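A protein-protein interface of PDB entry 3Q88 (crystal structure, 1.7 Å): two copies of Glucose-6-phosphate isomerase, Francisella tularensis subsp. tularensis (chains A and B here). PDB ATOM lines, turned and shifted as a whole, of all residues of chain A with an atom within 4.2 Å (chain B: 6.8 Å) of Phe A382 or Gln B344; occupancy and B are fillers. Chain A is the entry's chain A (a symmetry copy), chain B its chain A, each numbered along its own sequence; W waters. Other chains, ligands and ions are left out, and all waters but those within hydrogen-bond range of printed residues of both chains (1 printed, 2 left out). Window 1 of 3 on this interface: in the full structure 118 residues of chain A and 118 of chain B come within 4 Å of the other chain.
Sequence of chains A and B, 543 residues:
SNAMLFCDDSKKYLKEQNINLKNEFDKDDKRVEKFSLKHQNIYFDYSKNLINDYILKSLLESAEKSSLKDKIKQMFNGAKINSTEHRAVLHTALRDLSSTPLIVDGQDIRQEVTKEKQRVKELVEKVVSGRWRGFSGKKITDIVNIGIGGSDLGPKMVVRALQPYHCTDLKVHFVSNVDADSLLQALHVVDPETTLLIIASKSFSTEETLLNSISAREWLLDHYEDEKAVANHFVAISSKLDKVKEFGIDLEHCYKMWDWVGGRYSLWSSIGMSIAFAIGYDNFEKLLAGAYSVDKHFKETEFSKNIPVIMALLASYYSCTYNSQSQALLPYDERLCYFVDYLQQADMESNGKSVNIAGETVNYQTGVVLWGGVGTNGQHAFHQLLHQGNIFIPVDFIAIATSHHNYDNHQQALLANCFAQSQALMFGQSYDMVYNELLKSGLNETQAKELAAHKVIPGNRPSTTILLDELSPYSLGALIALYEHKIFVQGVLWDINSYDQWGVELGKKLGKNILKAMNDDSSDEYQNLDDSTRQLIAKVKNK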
ATOM      1  N   LEU A 330     -28.871  -9.405 -22.073  1.00  0.00           N
ATOM      2  CA  LEU A 330     -27.783  -8.945 -22.919  1.00  0.00           C
ATOM      3  C   LEU A 330     -28.159  -9.094 -24.410  1.00  0.00           C
ATOM      4  O   LEU A 330     -27.943 -10.162 -25.034  1.00  0.00           O
ATOM      5  CB  LEU A 330     -26.508  -9.759 -22.648  1.00  0.00           C
ATOM      6  CG  LEU A 330     -26.115  -9.933 -21.172  1.00  0.00           C
ATOM      7  CD1 LEU A 330     -24.866 -10.758 -20.985  1.00  0.00           C
ATOM      8  CD2 LEU A 330     -25.947  -8.470 -20.508  1.00  0.00           C
ATOM      9  N   TRP A 371     -31.457  -5.771 -15.375  1.00  0.00           N
ATOM     10  CA  TRP A 371     -30.460  -4.846 -15.900  1.00  0.00           C
ATOM     11  C   TRP A 371     -29.773  -5.522 -17.048  1.00  0.00           C
ATOM     12  O   TRP A 371     -30.049  -6.703 -17.355  1.00  0.00           O
ATOM     13  CB  TRP A 371     -29.447  -4.376 -14.802  1.00  0.00           C
ATOM     14  CG  TRP A 371     -28.611  -5.506 -14.299  1.00  0.00           C
ATOM     15  CD1 TRP A 371     -29.001  -6.483 -13.481  1.00  0.00           C
ATOM     16  CD2 TRP A 371     -27.286  -5.827 -14.733  1.00  0.00           C
ATOM     17  NE1 TRP A 371     -27.985  -7.407 -13.281  1.00  0.00           N
ATOM     18  CE2 TRP A 371     -26.906  -7.018 -14.045  1.00  0.00           C
ATOM     19  CE3 TRP A 371     -26.357  -5.190 -15.545  1.00  0.00           C
ATOM     20  CZ2 TRP A 371     -25.647  -7.600 -14.207  1.00  0.00           C
ATOM     21  CZ3 TRP A 371     -25.124  -5.781 -15.724  1.00  0.00           C
ATOM     22  CH2 TRP A 371     -24.775  -6.961 -15.087  1.00  0.00           C
ATOM     23  N   GLY A 372     -28.828  -4.816 -17.686  1.00  0.00           N
ATOM     24  CA  GLY A 372     -28.051  -5.493 -18.737  1.00  0.00           C
ATOM     25  C   GLY A 372     -27.467  -4.480 -19.667  1.00  0.00           C
ATOM     26  O   GLY A 372     -27.095  -3.388 -19.212  1.00  0.00           O
ATOM     27  N   GLY A 373     -27.284  -4.856 -20.916  1.00  0.00           N
ATOM     28  CA  GLY A 373     -26.579  -4.022 -21.851  1.00  0.00           C
ATOM     29  C   GLY A 373     -26.318  -4.685 -23.185  1.00  0.00           C
ATOM     30  O   GLY A 373     -26.212  -5.903 -23.231  1.00  0.00           O
ATOM     31  N   GLY A 378     -21.074  -4.515 -23.861  1.00  0.00           N
ATOM     32  CA  GLY A 378     -21.099  -4.880 -22.455  1.00  0.00           C
ATOM     33  C   GLY A 378     -19.908  -5.735 -22.051  1.00  0.00           C
ATOM     34  O   GLY A 378     -19.493  -5.741 -20.889  1.00  0.00           O
ATOM     35  N   ALA A 381     -17.452  -3.601 -20.510  1.00  0.00           N
ATOM     36  CA  ALA A 381     -17.984  -2.795 -19.426  1.00  0.00           C
ATOM     37  C   ALA A 381     -18.268  -3.523 -18.155  1.00  0.00           C
ATOM     38  O   ALA A 381     -17.675  -3.178 -17.120  1.00  0.00           O
ATOM     39  CB  ALA A 381     -19.259  -2.045 -19.897  1.00  0.00           C
ATOM     40  N   PHE A 382     -19.119  -4.539 -18.186  1.00  0.00           N
ATOM     41  CA  PHE A 382     -19.493  -5.238 -16.983  1.00  0.00           C
ATOM     42  C   PHE A 382     -19.390  -6.747 -17.030  1.00  0.00           C
ATOM     43  O   PHE A 382     -19.598  -7.433 -15.999  1.00  0.00           O
ATOM     44  CB  PHE A 382     -20.900  -4.805 -16.567  1.00  0.00           C
ATOM     45  CG  PHE A 382     -21.946  -5.011 -17.654  1.00  0.00           C
ATOM     46  CD1 PHE A 382     -22.413  -6.270 -17.940  1.00  0.00           C
ATOM     47  CD2 PHE A 382     -22.379  -3.938 -18.422  1.00  0.00           C
ATOM     48  CE1 PHE A 382     -23.313  -6.495 -18.892  1.00  0.00           C
ATOM     49  CE2 PHE A 382     -23.298  -4.140 -19.445  1.00  0.00           C
ATOM     50  CZ  PHE A 382     -23.740  -5.423 -19.703  1.00  0.00           C
ATOM     51  N   HIS A 383     -19.066  -7.310 -18.197  1.00  0.00           N
ATOM     52  CA  HIS A 383     -18.872  -8.774 -18.223  1.00  0.00           C
ATOM     53  C   HIS A 383     -17.729  -9.236 -17.328  1.00  0.00           C
ATOM     54  O   HIS A 383     -17.822 -10.354 -16.810  1.00  0.00           O
ATOM     55  CB  HIS A 383     -18.702  -9.372 -19.622  1.00  0.00           C
ATOM     56  CG  HIS A 383     -19.932  -9.349 -20.453  1.00  0.00           C
ATOM     57  ND1 HIS A 383     -20.192 -10.287 -21.410  1.00  0.00           N
ATOM     58  CD2 HIS A 383     -20.918  -8.426 -20.551  1.00  0.00           C
ATOM     59  CE1 HIS A 383     -21.308  -9.958 -22.043  1.00  0.00           C
ATOM     60  NE2 HIS A 383     -21.774  -8.841 -21.532  1.00  0.00           N
ATOM     61  N   GLN A 384     -16.737  -8.402 -17.067  1.00  0.00           N
ATOM     62  CA  GLN A 384     -15.735  -8.776 -16.016  1.00  0.00           C
ATOM     63  C   GLN A 384     -16.394  -9.254 -14.734  1.00  0.00           C
ATOM     64  O   GLN A 384     -15.914 -10.213 -14.131  1.00  0.00           O
ATOM     65  CB  GLN A 384     -14.855  -7.577 -15.702  1.00  0.00           C
ATOM     66  CG  GLN A 384     -14.002  -7.606 -14.488  1.00  0.00           C
ATOM     67  CD  GLN A 384     -12.961  -8.642 -14.494  1.00  0.00           C
ATOM     68  OE1 GLN A 384     -12.379  -8.929 -15.528  1.00  0.00           O
ATOM     69  NE2 GLN A 384     -12.726  -9.250 -13.279  1.00  0.00           N
ATOM     70  N   LEU A 385     -17.441  -8.546 -14.286  1.00  0.00           N
ATOM     71  CA  LEU A 385     -18.151  -8.930 -13.087  1.00  0.00           C
ATOM     72  C   LEU A 385     -18.921 -10.238 -13.271  1.00  0.00           C
ATOM     73  O   LEU A 385     -18.946 -11.085 -12.365  1.00  0.00           O
ATOM     74  CB  LEU A 385     -19.007  -7.779 -12.529  1.00  0.00           C
ATOM     75  CG  LEU A 385     -19.726  -8.053 -11.175  1.00  0.00           C
ATOM     76  CD1 LEU A 385     -19.762  -6.744 -10.322  1.00  0.00           C
ATOM     77  CD2 LEU A 385     -21.124  -8.684 -11.376  1.00  0.00           C
ATOM     78  N   LEU A 386     -19.574 -10.395 -14.429  1.00  0.00           N
ATOM     79  CA  LEU A 386     -20.245 -11.627 -14.728  1.00  0.00           C
ATOM     80  C   LEU A 386     -19.287 -12.848 -14.667  1.00  0.00           C
ATOM     81  O   LEU A 386     -19.710 -13.928 -14.247  1.00  0.00           O
ATOM     82  CB  LEU A 386     -20.985 -11.585 -16.080  1.00  0.00           C
ATOM     83  CG  LEU A 386     -22.052 -10.518 -16.216  1.00  0.00           C
ATOM     84  CD1 LEU A 386     -22.669 -10.561 -17.635  1.00  0.00           C
ATOM     85  CD2 LEU A 386     -23.146 -10.706 -15.177  1.00  0.00           C
ATOM     86  N   LEU B 153     -17.343   4.873 -24.300  1.00  0.00           N
ATOM     87  CA  LEU B 153     -18.453   5.238 -23.456  1.00  0.00           C
ATOM     88  C   LEU B 153     -18.224   6.583 -22.707  1.00  0.00           C
ATOM     89  O   LEU B 153     -19.128   7.404 -22.586  1.00  0.00           O
ATOM     90  CB  LEU B 153     -18.713   4.119 -22.468  1.00  0.00           C
ATOM     91  CG  LEU B 153     -19.960   4.219 -21.625  1.00  0.00           C
ATOM     92  CD1 LEU B 153     -21.173   4.759 -22.422  1.00  0.00           C
ATOM     93  CD2 LEU B 153     -20.310   2.868 -21.045  1.00  0.00           C
ATOM     94  N   LEU B 329     -28.658   4.141  -9.218  1.00  0.00           N
ATOM     95  CA  LEU B 329     -28.164   5.489  -9.488  1.00  0.00           C
ATOM     96  C   LEU B 329     -29.206   6.195 -10.381  1.00  0.00           C
ATOM     97  O   LEU B 329     -29.490   5.710 -11.484  1.00  0.00           O
ATOM     98  CB  LEU B 329     -26.820   5.416 -10.173  1.00  0.00           C
ATOM     99  CG  LEU B 329     -26.156   6.716 -10.604  1.00  0.00           C
ATOM    100  CD1 LEU B 329     -25.999   7.681  -9.415  1.00  0.00           C
ATOM    101  CD2 LEU B 329     -24.784   6.432 -11.222  1.00  0.00           C
ATOM    102  N   PHE B 339     -24.895   8.281 -18.094  1.00  0.00           N
ATOM    103  CA  PHE B 339     -24.093   8.284 -16.900  1.00  0.00           C
ATOM    104  C   PHE B 339     -24.123   6.919 -16.197  1.00  0.00           C
ATOM    105  O   PHE B 339     -23.094   6.446 -15.729  1.00  0.00           O
ATOM    106  CB  PHE B 339     -24.555   9.448 -16.019  1.00  0.00           C
ATOM    107  CG  PHE B 339     -23.656   9.729 -14.850  1.00  0.00           C
ATOM    108  CD1 PHE B 339     -22.428  10.350 -15.016  1.00  0.00           C
ATOM    109  CD2 PHE B 339     -24.080   9.422 -13.568  1.00  0.00           C
ATOM    110  CE1 PHE B 339     -21.579  10.586 -13.896  1.00  0.00           C
ATOM    111  CE2 PHE B 339     -23.261   9.683 -12.460  1.00  0.00           C
ATOM    112  CZ  PHE B 339     -22.021  10.260 -12.633  1.00  0.00           C
ATOM    113  N   VAL B 340     -25.289   6.311 -16.036  1.00  0.00           N
ATOM    114  CA  VAL B 340     -25.310   4.957 -15.433  1.00  0.00           C
ATOM    115  C   VAL B 340     -24.484   3.964 -16.230  1.00  0.00           C
ATOM    116  O   VAL B 340     -23.693   3.204 -15.658  1.00  0.00           O
ATOM    117  CB  VAL B 340     -26.747   4.438 -15.314  1.00  0.00           C
ATOM    118  CG1 VAL B 340     -26.745   2.951 -14.954  1.00  0.00           C
ATOM    119  CG2 VAL B 340     -27.518   5.244 -14.235  1.00  0.00           C
ATOM    120  N   ASP B 341     -24.616   3.987 -17.574  1.00  0.00           N
ATOM    121  CA  ASP B 341     -23.865   3.080 -18.449  1.00  0.00           C
ATOM    122  C   ASP B 341     -22.331   3.228 -18.202  1.00  0.00           C
ATOM    123  O   ASP B 341     -21.568   2.248 -18.090  1.00  0.00           O
ATOM    124  CB  ASP B 341     -24.107   3.323 -19.919  1.00  0.00           C
ATOM    125  CG  ASP B 341     -25.579   2.897 -20.382  1.00  0.00           C
ATOM    126  OD1 ASP B 341     -26.279   2.195 -19.657  1.00  0.00           O
ATOM    127  OD2 ASP B 341     -25.918   3.209 -21.495  1.00  0.00           O
ATOM    128  N   TYR B 342     -21.901   4.488 -18.105  1.00  0.00           N
ATOM    129  CA  TYR B 342     -20.496   4.832 -17.880  1.00  0.00           C
ATOM    130  C   TYR B 342     -20.031   4.300 -16.535  1.00  0.00           C
ATOM    131  O   TYR B 342     -18.995   3.630 -16.448  1.00  0.00           O
ATOM    132  CB  TYR B 342     -20.288   6.343 -17.983  1.00  0.00           C
ATOM    133  CG  TYR B 342     -18.823   6.696 -17.768  1.00  0.00           C
ATOM    134  CD1 TYR B 342     -17.888   6.540 -18.787  1.00  0.00           C
ATOM    135  CD2 TYR B 342     -18.375   7.078 -16.520  1.00  0.00           C
ATOM    136  CE1 TYR B 342     -16.524   6.797 -18.544  1.00  0.00           C
ATOM    137  CE2 TYR B 342     -17.006   7.383 -16.289  1.00  0.00           C
ATOM    138  CZ  TYR B 342     -16.114   7.242 -17.305  1.00  0.00           C
ATOM    139  OH  TYR B 342     -14.789   7.485 -17.096  1.00  0.00           O
ATOM    140  N   LEU B 343     -20.822   4.550 -15.504  1.00  0.00           N
ATOM    141  CA  LEU B 343     -20.396   4.144 -14.136  1.00  0.00           C
ATOM    142  C   LEU B 343     -20.490   2.648 -13.971  1.00  0.00           C
ATOM    143  O   LEU B 343     -19.696   2.068 -13.221  1.00  0.00           O
ATOM    144  CB  LEU B 343     -21.138   4.929 -13.107  1.00  0.00           C
ATOM    145  CG  LEU B 343     -20.565   6.379 -12.931  1.00  0.00           C
ATOM    146  CD1 LEU B 343     -21.287   7.080 -11.793  1.00  0.00           C
ATOM    147  CD2 LEU B 343     -19.059   6.573 -12.719  1.00  0.00           C
ATOM    148  N   GLN B 344     -21.394   1.965 -14.692  1.00  0.00           N
ATOM    149  CA  GLN B 344     -21.340   0.514 -14.742  1.00  0.00           C
ATOM    150  C   GLN B 344     -20.009  -0.032 -15.115  1.00  0.00           C
ATOM    151  O   GLN B 344     -19.497  -0.939 -14.451  1.00  0.00           O
ATOM    152  CB  GLN B 344     -22.375  -0.072 -15.713  1.00  0.00           C
ATOM    153  CG  GLN B 344     -23.684  -0.053 -15.255  1.00  0.00           C
ATOM    154  CD  GLN B 344     -24.607  -0.770 -16.229  1.00  0.00           C
ATOM    155  OE1 GLN B 344     -24.323  -0.829 -17.467  1.00  0.00           O
ATOM    156  NE2 GLN B 344     -25.696  -1.354 -15.682  1.00  0.00           N
ATOM    157  N   GLN B 345     -19.407   0.535 -16.176  1.00  0.00           N
ATOM    158  CA  GLN B 345     -18.085   0.150 -16.584  1.00  0.00           C
ATOM    159  C   GLN B 345     -17.049   0.475 -15.499  1.00  0.00           C
ATOM    160  O   GLN B 345     -16.325  -0.409 -15.001  1.00  0.00           O
ATOM    161  CB  GLN B 345     -17.659   0.794 -17.925  1.00  0.00           C
ATOM    162  CG  GLN B 345     -16.275   0.312 -18.158  1.00  0.00           C
ATOM    163  CD  GLN B 345     -15.699   0.550 -19.484  1.00  0.00           C
ATOM    164  OE1 GLN B 345     -16.326   1.273 -20.291  1.00  0.00           O
ATOM    165  NE2 GLN B 345     -14.470  -0.132 -19.762  1.00  0.00           N
ATOM    166  N   ALA B 346     -17.028   1.702 -15.034  1.00  0.00           N
ATOM    167  CA  ALA B 346     -16.023   2.074 -14.070  1.00  0.00           C
ATOM    168  C   ALA B 346     -16.076   1.255 -12.793  1.00  0.00           C
ATOM    169  O   ALA B 346     -15.034   0.889 -12.227  1.00  0.00           O
ATOM    170  CB  ALA B 346     -16.136   3.571 -13.718  1.00  0.00           C
ATOM    171  N   ASP B 347     -17.282   1.034 -12.291  1.00  0.00           N
ATOM    172  CA  ASP B 347     -17.467   0.338 -11.030  1.00  0.00           C
ATOM    173  C   ASP B 347     -17.312  -1.185 -11.202  1.00  0.00           C
ATOM    174  O   ASP B 347     -16.441  -1.792 -10.553  1.00  0.00           O
ATOM    175  CB  ASP B 347     -18.833   0.684 -10.512  1.00  0.00           C
ATOM    176  CG  ASP B 347     -19.135   0.223  -9.147  1.00  0.00           C
ATOM    177  OD1 ASP B 347     -18.406  -0.610  -8.576  1.00  0.00           O
ATOM    178  OD2 ASP B 347     -20.232   0.674  -8.631  1.00  0.00           O
ATOM    179  N   MET B 348     -18.160  -1.799 -12.052  1.00  0.00           N
ATOM    180  CA  MET B 348     -18.256  -3.256 -12.121  1.00  0.00           C
ATOM    181  C   MET B 348     -17.020  -3.907 -12.705  1.00  0.00           C
ATOM    182  O   MET B 348     -16.605  -4.948 -12.181  1.00  0.00           O
ATOM    183  CB  MET B 348     -19.493  -3.699 -12.858  1.00  0.00           C
ATOM    184  CG  MET B 348     -20.761  -3.183 -12.175  1.00  0.00           C
ATOM    185  SD  MET B 348     -22.311  -3.616 -13.085  1.00  0.00           S
ATOM    186  CE  MET B 348     -22.380  -5.318 -12.979  1.00  0.00           C
ATOM    187  N   GLU B 349     -16.394  -3.287 -13.715  1.00  0.00           N
ATOM    188  CA  GLU B 349     -15.178  -3.875 -14.248  1.00  0.00           C
ATOM    189  C   GLU B 349     -13.999  -3.708 -13.249  1.00  0.00           C
ATOM    190  O   GLU B 349     -13.078  -4.522 -13.248  1.00  0.00           O
ATOM    191  CB  GLU B 349     -14.800  -3.247 -15.577  1.00  0.00           C
ATOM    192  CG  GLU B 349     -13.784  -4.051 -16.301  1.00  0.00           C
ATOM    193  CD  GLU B 349     -13.590  -3.622 -17.745  1.00  0.00           C
ATOM    194  OE1 GLU B 349     -13.054  -2.532 -17.963  1.00  0.00           O
ATOM    195  OE2 GLU B 349     -13.972  -4.404 -18.640  1.00  0.00           O
ATOM    196  N   SER B 350     -14.032  -2.663 -12.406  1.00  0.00           N
ATOM    197  CA  SER B 350     -13.040  -2.516 -11.373  1.00  0.00           C
ATOM    198  C   SER B 350     -13.167  -3.499 -10.245  1.00  0.00           C
ATOM    199  O   SER B 350     -12.165  -4.165  -9.834  1.00  0.00           O
ATOM    200  CB  SER B 350     -13.049  -1.106 -10.787  1.00  0.00           C
ATOM    201  OG  SER B 350     -12.686  -0.136 -11.792  1.00  0.00           O
ATOM    202  N   VAL B 369     -23.846  -5.101  -8.566  1.00  0.00           N
ATOM    203  CA  VAL B 369     -24.423  -4.578  -9.789  1.00  0.00           C
ATOM    204  C   VAL B 369     -24.790  -3.095  -9.616  1.00  0.00           C
ATOM    205  O   VAL B 369     -25.505  -2.708  -8.665  1.00  0.00           O
ATOM    206  CB  VAL B 369     -25.670  -5.386 -10.177  1.00  0.00           C
ATOM    207  CG1 VAL B 369     -26.367  -4.732 -11.406  1.00  0.00           C
ATOM    208  CG2 VAL B 369     -25.264  -6.869 -10.503  1.00  0.00           C
ATOM    209  N   LEU B 370     -24.369  -2.256 -10.541  1.00  0.00           N
ATOM    210  CA  LEU B 370     -24.774  -0.883 -10.601  1.00  0.00           C
ATOM    211  C   LEU B 370     -25.810  -0.747 -11.739  1.00  0.00           C
ATOM    212  O   LEU B 370     -25.597  -1.217 -12.850  1.00  0.00           O
ATOM    213  CB  LEU B 370     -23.607   0.044 -10.906  1.00  0.00           C
ATOM    214  CG  LEU B 370     -23.886   1.549 -10.781  1.00  0.00           C
ATOM    215  CD1 LEU B 370     -24.348   2.004  -9.412  1.00  0.00           C
ATOM    216  CD2 LEU B 370     -22.654   2.357 -11.221  1.00  0.00           C
ATOM    217  N   TRP B 371     -26.955  -0.098 -11.442  1.00  0.00           N
ATOM    218  CA  TRP B 371     -28.017   0.076 -12.424  1.00  0.00           C
ATOM    219  C   TRP B 371     -28.741   1.346 -12.093  1.00  0.00           C
ATOM    220  O   TRP B 371     -28.435   2.013 -11.081  1.00  0.00           O
ATOM    221  CB  TRP B 371     -28.985  -1.156 -12.478  1.00  0.00           C
ATOM    222  CG  TRP B 371     -29.743  -1.320 -11.203  1.00  0.00           C
ATOM    223  CD1 TRP B 371     -29.266  -1.781 -10.046  1.00  0.00           C
ATOM    224  CD2 TRP B 371     -31.076  -0.864 -10.954  1.00  0.00           C
ATOM    225  NE1 TRP B 371     -30.230  -1.729  -9.048  1.00  0.00           N
ATOM    226  CE2 TRP B 371     -31.366  -1.167  -9.590  1.00  0.00           C
ATOM    227  CE3 TRP B 371     -32.075  -0.327 -11.754  1.00  0.00           C
ATOM    228  CZ2 TRP B 371     -32.607  -0.886  -9.014  1.00  0.00           C
ATOM    229  CZ3 TRP B 371     -33.291  -0.027 -11.176  1.00  0.00           C
ATOM    230  CH2 TRP B 371     -33.554  -0.283  -9.840  1.00  0.00           C
ATOM    231  N   GLY B 372     -29.749   1.695 -12.905  1.00  0.00           N
ATOM    232  CA  GLY B 372     -30.556   2.870 -12.538  1.00  0.00           C
ATOM    233  C   GLY B 372     -31.235   3.418 -13.753  1.00  0.00           C
ATOM    234  O   GLY B 372     -31.626   2.633 -14.629  1.00  0.00           O
ATOM    235  N   VAL B 504     -12.011 -10.974 -18.614  1.00  0.00           N
ATOM    236  CA  VAL B 504     -12.484 -10.825 -19.999  1.00  0.00           C
ATOM    237  C   VAL B 504     -11.655 -11.619 -20.976  1.00  0.00           C
ATOM    238  O   VAL B 504     -12.037 -11.762 -22.124  1.00  0.00           O
ATOM    239  CB  VAL B 504     -12.545  -9.343 -20.410  1.00  0.00           C
ATOM    240  CG1 VAL B 504     -13.476  -8.552 -19.360  1.00  0.00           C
ATOM    241  CG2 VAL B 504     -11.144  -8.713 -20.535  1.00  0.00           C
HETATM  242  O   HOH W   1     -28.248  -1.991 -17.194  1.00  0.00           O
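Water W1 lies within hydrogen-bond range of O of Gly A372 and NE2 of Gln B344.
Hydrophobic or aromatic side chains of chain B within 4 Å of the printed part of chain A: Met B348, Val B369, Trp B371 and Val B504. Among the printed residues, 12 pairs touch across the chains.
Among the printed residues, merely in contact across the chains: Trp A371 with Gln B344 (3.9 Å), Trp A371 with Met B348 (3.6 Å), Trp A371 with Val B369 (3.5 Å), Trp A371 with Trp B371 (3.998 Å), Ala A381 with Gln B344 (3.9 Å), Ala A381 with Gln B345 (3.4 Å), Ala A381 with Glu B349 (3.3 Å), Phe A382 with Gln B344 (3.8 Å), Phe A382 with Met B348 (3.9 Å), Gln A384 with Glu B349 (3.4 Å), Gln A384 with Val B504 (3.7 Å) and Leu A385 with Met B348 (3.7 Å).
NE2 of Gln B345 is in hydrogen-bond range of OE1 of Glu B349 (3.3 Å). N of Leu B370 lies within hydrogen-bond range of SD of Met B348, at 3.5 Å. The side-chain amide nitrogen (NE2) of Gln B344 sits at hydrogen-bond distance from the backbone carbonyl oxygen (O) of Leu B370 (2.8 Å). The backbone NH (N) of Leu B329 sits at hydrogen-bond distance from the backbone carbonyl oxygen (O) of Trp B371, 2.8 Å away.
Trp B371 touches its own counterpart, Trp A371. Positions printed for both chains: 371 and 372.
Phe A382 touches two residues of chain B. Of the printed residues of chain A, Met B348 touches Trp A371 (3.6 Å), Phe A382 (3.9 Å) and Leu A385 (3.7 Å). Of the printed residues of chain A, Val B504 touches Gln A384. Of the printed residues of chain B, Trp A371 touches Gln B344 (3.9 Å), Met B348 (3.6 Å), Val B369 (3.5 Å) and Trp B371 (3.998 Å). Leu A330 touches none of the printed residues of chain B. The nearest residue of chain B that does not touch Phe A382 is Glu B349 (4.9 Å).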
